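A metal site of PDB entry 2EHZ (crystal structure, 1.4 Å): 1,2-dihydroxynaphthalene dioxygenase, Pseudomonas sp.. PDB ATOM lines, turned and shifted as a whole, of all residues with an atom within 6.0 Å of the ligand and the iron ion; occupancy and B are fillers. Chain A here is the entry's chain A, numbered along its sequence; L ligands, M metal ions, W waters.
OH of Tyr 256 lies close to O1 of the ligand, at 2.6 Å.
O2 of the ligand lies close to NE2 of His 200 (2.6 Å).
An oxygen (O2) of the ligand sits close to a ring nitrogen (NE2) of His 247 (3.5 Å).
The side-chain carboxylate of Glu 266 is in hydrogen-bond range of the side-chain hydroxyl of Tyr 256 (3.1 Å).
O of His 152 is in hydrogen-bond range of N of Met 217 (2.8 Å).
O of His 215 is in hydrogen-bond range of N of Ile 154 (3.1 Å).
NE2 of His 247 sits close to OH of Tyr 256, at 3.2 Å.
The side-chain carboxylate (OD2) of Asp 284 is in hydrogen-bond range of a ring nitrogen (ND1) of His 247, 2.8 Å away.
The backbone NH (N) of Asn 249 lies within hydrogen-bond range of the side-chain hydroxyl (OH) of Tyr 178 (3.0 Å).
The backbone NH (N) of Ala 248 is in hydrogen-bond range of the side-chain hydroxyl (OH) of Tyr 178 (3.1 Å).
The backbone NH (N) of Asp 284 lies within hydrogen-bond range of the backbone carbonyl oxygen (O) of Leu 301, at 2.8 Å.
Residues that only touch the ligand: Asn 249 (3.3 Å), Phe 192 (3.5 Å), Tyr 178 (3.6 Å), Leu 301 (3.9 Å) and Ile 154 (3.98 Å).
Hydrophobic or aromatic side chains within 4 Å of the ligand: His 152, Ile 154, Tyr 178, Phe 192, His 200, His 215, His 247, Tyr 256 and Leu 301.
The nearest printed residue that does not touch the ligand is Leu 190 (4.3 Å).
Merely in contact with the iron ion: Tyr 256 (3.6 Å).
Of the 18 residues printed, 4 come within 4 Å of the iron ion.
The nearest printed residue that does not touch the iron ion is His 200 (4.2 Å).
The iron ion is bound by the side-chain carboxylate (OE1) of Glu 266, at 2.0 Å.
O1 of the ligand binds the iron ion, at 2.1 Å.
A ring nitrogen (NE2) of His 152 is bound to the iron ion (2.2 Å).
NE2 of His 215 binds the iron ion (2.2 Å).
The iron ion is bound by an oxygen (O2) of the ligand, 2.2 Å away.
The iron ion has five donor atoms within binding distance.
Water W1 bridges OD2 of Asp 250 (2.8 Å) and OE2 of Glu 266 (3.4 Å).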
ATOM      1  N   HIS A 152       5.703 -33.880  -8.483  1.00  0.00           N
ATOM      2  CA  HIS A 152       5.672 -32.683  -9.333  1.00  0.00           C
ATOM      3  C   HIS A 152       7.069 -32.193  -9.645  1.00  0.00           C
ATOM      4  O   HIS A 152       8.014 -32.532  -8.933  1.00  0.00           O
ATOM      5  CB  HIS A 152       4.822 -31.545  -8.735  1.00  0.00           C
ATOM      6  CG  HIS A 152       5.421 -30.835  -7.547  1.00  0.00           C
ATOM      7  ND1 HIS A 152       4.869 -30.928  -6.293  1.00  0.00           N
ATOM      8  CD2 HIS A 152       6.453 -29.963  -7.435  1.00  0.00           C
ATOM      9  CE1 HIS A 152       5.552 -30.170  -5.452  1.00  0.00           C
ATOM     10  NE2 HIS A 152       6.520 -29.572  -6.127  1.00  0.00           N
ATOM     11  N   ILE A 154       9.196 -28.390 -10.852  1.00  0.00           N
ATOM     12  CA  ILE A 154       9.360 -27.058 -11.435  1.00  0.00           C
ATOM     13  C   ILE A 154      10.384 -27.176 -12.543  1.00  0.00           C
ATOM     14  O   ILE A 154      11.470 -27.731 -12.339  1.00  0.00           O
ATOM     15  CB  ILE A 154       9.792 -25.984 -10.412  1.00  0.00           C
ATOM     16  CG1 ILE A 154       8.603 -25.624  -9.515  1.00  0.00           C
ATOM     17  CG2 ILE A 154      10.336 -24.723 -11.118  1.00  0.00           C
ATOM     18  CD1 ILE A 154       8.855 -24.405  -8.632  1.00  0.00           C
ATOM     19  N   TYR A 178       1.959 -17.419  -6.591  1.00  0.00           N
ATOM     20  CA  TYR A 178       2.859 -16.685  -5.709  1.00  0.00           C
ATOM     21  C   TYR A 178       3.391 -15.453  -6.381  1.00  0.00           C
ATOM     22  O   TYR A 178       3.811 -15.494  -7.543  1.00  0.00           O
ATOM     23  CB  TYR A 178       4.048 -17.535  -5.296  1.00  0.00           C
ATOM     24  CG  TYR A 178       3.705 -18.637  -4.336  1.00  0.00           C
ATOM     25  CD1 TYR A 178       3.102 -19.804  -4.772  1.00  0.00           C
ATOM     26  CD2 TYR A 178       4.007 -18.519  -2.977  1.00  0.00           C
ATOM     27  CE1 TYR A 178       2.792 -20.848  -3.890  1.00  0.00           C
ATOM     28  CE2 TYR A 178       3.702 -19.558  -2.083  1.00  0.00           C
ATOM     29  CZ  TYR A 178       3.102 -20.693  -2.550  1.00  0.00           C
ATOM     30  OH  TYR A 178       2.817 -21.722  -1.676  1.00  0.00           O
ATOM     31  N   ILE A 180       6.322 -13.309  -5.085  1.00  0.00           N
ATOM     32  CA  ILE A 180       7.338 -13.331  -4.022  1.00  0.00           C
ATOM     33  C   ILE A 180       8.337 -12.189  -4.200  1.00  0.00           C
ATOM     34  O   ILE A 180       8.963 -12.081  -5.252  1.00  0.00           O
ATOM     35  CB  ILE A 180       8.073 -14.701  -3.964  1.00  0.00           C
ATOM     36  CG1 ILE A 180       7.088 -15.826  -3.620  1.00  0.00           C
ATOM     37  CG2 ILE A 180       9.237 -14.666  -2.950  1.00  0.00           C
ATOM     38  CD1 ILE A 180       7.625 -17.236  -3.835  1.00  0.00           C
ATOM     39  N   LEU A 190       5.226 -17.033  -9.728  1.00  0.00           N
ATOM     40  CA  LEU A 190       5.304 -18.471  -9.967  1.00  0.00           C
ATOM     41  C   LEU A 190       3.919 -19.034 -10.223  1.00  0.00           C
ATOM     42  O   LEU A 190       2.979 -18.724  -9.482  1.00  0.00           O
ATOM     43  CB  LEU A 190       5.951 -19.196  -8.789  1.00  0.00           C
ATOM     44  CG  LEU A 190       7.395 -18.812  -8.447  1.00  0.00           C
ATOM     45  CD1 LEU A 190       7.886 -19.638  -7.279  1.00  0.00           C
ATOM     46  CD2 LEU A 190       8.328 -18.974  -9.648  1.00  0.00           C
ATOM     47  N   PHE A 192       1.417 -22.471 -11.042  1.00  0.00           N
ATOM     48  CA  PHE A 192       1.296 -23.865 -10.596  1.00  0.00           C
ATOM     49  C   PHE A 192       0.072 -24.479 -11.235  1.00  0.00           C
ATOM     50  O   PHE A 192      -1.018 -23.920 -11.145  1.00  0.00           O
ATOM     51  CB  PHE A 192       1.149 -23.947  -9.070  1.00  0.00           C
ATOM     52  CG  PHE A 192       2.349 -23.451  -8.324  1.00  0.00           C
ATOM     53  CD1 PHE A 192       2.589 -22.090  -8.181  1.00  0.00           C
ATOM     54  CD2 PHE A 192       3.272 -24.347  -7.781  1.00  0.00           C
ATOM     55  CE1 PHE A 192       3.716 -21.630  -7.505  1.00  0.00           C
ATOM     56  CE2 PHE A 192       4.399 -23.888  -7.105  1.00  0.00           C
ATOM     57  CZ  PHE A 192       4.626 -22.529  -6.973  1.00  0.00           C
ATOM     58  N   HIS A 200      -0.293 -29.597  -7.305  1.00  0.00           N
ATOM     59  CA  HIS A 200       0.297 -29.237  -8.589  1.00  0.00           C
ATOM     60  C   HIS A 200       1.142 -30.395  -9.087  1.00  0.00           C
ATOM     61  O   HIS A 200       1.690 -31.145  -8.284  1.00  0.00           O
ATOM     62  CB  HIS A 200       1.112 -27.937  -8.535  1.00  0.00           C
ATOM     63  CG  HIS A 200       2.034 -27.817  -7.342  1.00  0.00           C
ATOM     64  ND1 HIS A 200       1.559 -27.559  -6.080  1.00  0.00           N
ATOM     65  CD2 HIS A 200       3.377 -27.891  -7.230  1.00  0.00           C
ATOM     66  CE1 HIS A 200       2.564 -27.494  -5.229  1.00  0.00           C
ATOM     67  NE2 HIS A 200       3.689 -27.687  -5.904  1.00  0.00           N
ATOM     68  N   HIS A 215      13.472 -28.635  -9.549  1.00  0.00           N
ATOM     69  CA  HIS A 215      13.328 -29.669  -8.531  1.00  0.00           C
ATOM     70  C   HIS A 215      12.250 -30.668  -8.882  1.00  0.00           C
ATOM     71  O   HIS A 215      11.333 -30.365  -9.654  1.00  0.00           O
ATOM     72  CB  HIS A 215      13.084 -29.080  -7.124  1.00  0.00           C
ATOM     73  CG  HIS A 215      11.707 -28.534  -6.911  1.00  0.00           C
ATOM     74  ND1 HIS A 215      11.360 -27.237  -7.234  1.00  0.00           N
ATOM     75  CD2 HIS A 215      10.600 -29.098  -6.368  1.00  0.00           C
ATOM     76  CE1 HIS A 215      10.099 -27.038  -6.909  1.00  0.00           C
ATOM     77  NE2 HIS A 215       9.610 -28.140  -6.374  1.00  0.00           N
ATOM     78  N   MET A 217       9.568 -33.110  -6.657  1.00  0.00           N
ATOM     79  CA  MET A 217       8.990 -33.361  -5.342  1.00  0.00           C
ATOM     80  C   MET A 217       8.437 -34.773  -5.318  1.00  0.00           C
ATOM     81  O   MET A 217       7.688 -35.164  -6.226  1.00  0.00           O
ATOM     82  CB  MET A 217       7.860 -32.353  -5.054  1.00  0.00           C
ATOM     83  CG  MET A 217       7.285 -32.398  -3.649  1.00  0.00           C
ATOM     84  SD  MET A 217       5.968 -33.611  -3.442  1.00  0.00           S
ATOM     85  CE  MET A 217       5.580 -33.334  -1.708  1.00  0.00           C
ATOM     86  N   HIS A 247       4.192 -25.159   2.524  1.00  0.00           N
ATOM     87  CA  HIS A 247       3.712 -24.362   1.398  1.00  0.00           C
ATOM     88  C   HIS A 247       2.304 -23.819   1.625  1.00  0.00           C
ATOM     89  O   HIS A 247       1.429 -24.547   2.099  1.00  0.00           O
ATOM     90  CB  HIS A 247       3.678 -25.201   0.131  1.00  0.00           C
ATOM     91  CG  HIS A 247       5.034 -25.549  -0.403  1.00  0.00           C
ATOM     92  ND1 HIS A 247       5.988 -24.586  -0.699  1.00  0.00           N
ATOM     93  CD2 HIS A 247       5.581 -26.737  -0.750  1.00  0.00           C
ATOM     94  CE1 HIS A 247       7.055 -25.182  -1.188  1.00  0.00           C
ATOM     95  NE2 HIS A 247       6.837 -26.482  -1.233  1.00  0.00           N
ATOM     96  N   ALA A 248       2.079 -22.559   1.230  1.00  0.00           N
ATOM     97  CA  ALA A 248       0.733 -21.979   1.303  1.00  0.00           C
ATOM     98  C   ALA A 248      -0.259 -22.637   0.341  1.00  0.00           C
ATOM     99  O   ALA A 248      -1.428 -22.789   0.683  1.00  0.00           O
ATOM    100  CB  ALA A 248       0.784 -20.476   1.090  1.00  0.00           C
ATOM    101  N   ASN A 249       0.193 -23.043  -0.857  1.00  0.00           N
ATOM    102  CA  ASN A 249      -0.740 -23.679  -1.785  1.00  0.00           C
ATOM    103  C   ASN A 249      -1.132 -25.115  -1.421  1.00  0.00           C
ATOM    104  O   ASN A 249      -2.319 -25.382  -1.219  1.00  0.00           O
ATOM    105  CB  ASN A 249      -0.318 -23.542  -3.277  1.00  0.00           C
ATOM    106  CG  ASN A 249       1.057 -24.135  -3.616  1.00  0.00           C
ATOM    107  OD1 ASN A 249       1.732 -24.756  -2.778  1.00  0.00           O
ATOM    108  ND2 ASN A 249       1.464 -23.960  -4.865  1.00  0.00           N
ATOM    109  N   ASP A 250      -0.170 -26.009  -1.302  1.00  0.00           N
ATOM    110  CA  ASP A 250      -0.518 -27.400  -1.088  1.00  0.00           C
ATOM    111  C   ASP A 250      -0.476 -27.865   0.365  1.00  0.00           C
ATOM    112  O   ASP A 250      -0.822 -29.010   0.652  1.00  0.00           O
ATOM    113  CB  ASP A 250       0.269 -28.341  -1.992  1.00  0.00           C
ATOM    114  CG  ASP A 250       1.725 -28.460  -1.618  1.00  0.00           C
ATOM    115  OD1 ASP A 250       2.165 -27.819  -0.634  1.00  0.00           O
ATOM    116  OD2 ASP A 250       2.433 -29.192  -2.335  1.00  0.00           O
ATOM    117  N   TYR A 256      14.139 -28.880   0.668  1.00  0.00           N
ATOM    118  CA  TYR A 256      14.780 -29.070  -0.629  1.00  0.00           C
ATOM    119  C   TYR A 256      16.261 -29.379  -0.429  1.00  0.00           C
ATOM    120  O   TYR A 256      16.987 -28.561   0.150  1.00  0.00           O
ATOM    121  CB  TYR A 256      14.655 -27.801  -1.473  1.00  0.00           C
ATOM    122  CG  TYR A 256      13.254 -27.337  -1.827  1.00  0.00           C
ATOM    123  CD1 TYR A 256      12.391 -26.794  -0.864  1.00  0.00           C
ATOM    124  CD2 TYR A 256      12.817 -27.363  -3.157  1.00  0.00           C
ATOM    125  CE1 TYR A 256      11.133 -26.321  -1.220  1.00  0.00           C
ATOM    126  CE2 TYR A 256      11.565 -26.902  -3.518  1.00  0.00           C
ATOM    127  CZ  TYR A 256      10.735 -26.363  -2.550  1.00  0.00           C
ATOM    128  OH  TYR A 256       9.490 -25.871  -2.878  1.00  0.00           O
ATOM    129  N   GLU A 266      12.794 -32.467  -3.537  1.00  0.00           N
ATOM    130  CA  GLU A 266      11.943 -31.911  -2.495  1.00  0.00           C
ATOM    131  C   GLU A 266      11.143 -33.058  -1.846  1.00  0.00           C
ATOM    132  O   GLU A 266      10.031 -33.357  -2.278  1.00  0.00           O
ATOM    133  CB  GLU A 266      10.992 -30.839  -3.086  1.00  0.00           C
ATOM    134  CG  GLU A 266      10.123 -30.156  -2.025  1.00  0.00           C
ATOM    135  CD  GLU A 266       9.033 -29.264  -2.583  1.00  0.00           C
ATOM    136  OE1 GLU A 266       8.753 -29.294  -3.792  1.00  0.00           O
ATOM    137  OE2 GLU A 266       8.427 -28.531  -1.759  1.00  0.00           O
ATOM    138  N   ASP A 284       5.143 -18.435   1.809  1.00  0.00           N
ATOM    139  CA  ASP A 284       4.686 -19.700   2.386  1.00  0.00           C
ATOM    140  C   ASP A 284       4.183 -19.491   3.826  1.00  0.00           C
ATOM    141  O   ASP A 284       4.240 -18.382   4.366  1.00  0.00           O
ATOM    142  CB  ASP A 284       5.811 -20.757   2.284  1.00  0.00           C
ATOM    143  CG  ASP A 284       5.746 -21.576   0.995  1.00  0.00           C
ATOM    144  OD1 ASP A 284       4.695 -21.578   0.314  1.00  0.00           O
ATOM    145  OD2 ASP A 284       6.733 -22.273   0.670  1.00  0.00           O
ATOM    146  N   LEU A 297      17.300 -22.646  -6.269  1.00  0.00           N
ATOM    147  CA  LEU A 297      16.528 -21.771  -5.392  1.00  0.00           C
ATOM    148  C   LEU A 297      17.434 -21.084  -4.378  1.00  0.00           C
ATOM    149  O   LEU A 297      17.909 -21.708  -3.422  1.00  0.00           O
ATOM    150  CB  LEU A 297      15.402 -22.556  -4.707  1.00  0.00           C
ATOM    151  CG  LEU A 297      14.425 -23.285  -5.644  1.00  0.00           C
ATOM    152  CD1 LEU A 297      13.663 -24.357  -4.895  1.00  0.00           C
ATOM    153  CD2 LEU A 297      13.467 -22.325  -6.331  1.00  0.00           C
ATOM    154  N   LEU A 301      11.258 -18.499   0.660  1.00  0.00           N
ATOM    155  CA  LEU A 301       9.866 -18.586   0.211  1.00  0.00           C
ATOM    156  C   LEU A 301       8.861 -18.005   1.204  1.00  0.00           C
ATOM    157  O   LEU A 301       7.674 -17.889   0.875  1.00  0.00           O
ATOM    158  CB  LEU A 301       9.490 -20.031  -0.154  1.00  0.00           C
ATOM    159  CG  LEU A 301      10.233 -20.696  -1.312  1.00  0.00           C
ATOM    160  CD1 LEU A 301       9.653 -22.076  -1.585  1.00  0.00           C
ATOM    161  CD2 LEU A 301      10.192 -19.840  -2.583  1.00  0.00           C
HETATM  162  C1  LIG L   1       6.256 -23.170  -3.933  1.00  0.00           C
HETATM  163  C2  LIG L   1       7.302 -23.925  -4.427  1.00  0.00           C
HETATM  164  C3  LIG L   1       7.128 -25.292  -4.600  1.00  0.00           C
HETATM  165  O1  LIG L   1       8.166 -26.051  -5.073  1.00  0.00           O
HETATM  166  C4  LIG L   1       5.936 -25.913  -4.286  1.00  0.00           C
HETATM  167  O2  LIG L   1       5.836 -27.268  -4.484  1.00  0.00           O
HETATM  168  C5  LIG L   1       4.856 -25.170  -3.782  1.00  0.00           C
HETATM  169  C6  LIG L   1       5.046 -23.785  -3.614  1.00  0.00           C
HETATM  170  C7  LIG L   1       6.444 -21.681  -3.735  1.00  0.00           C
HETATM  171 FE    FE M   1       7.800 -28.100  -5.143  1.00  0.00          FE
HETATM  172  O   HOH W   1       5.221 -29.487  -2.340  1.00  0.00           O
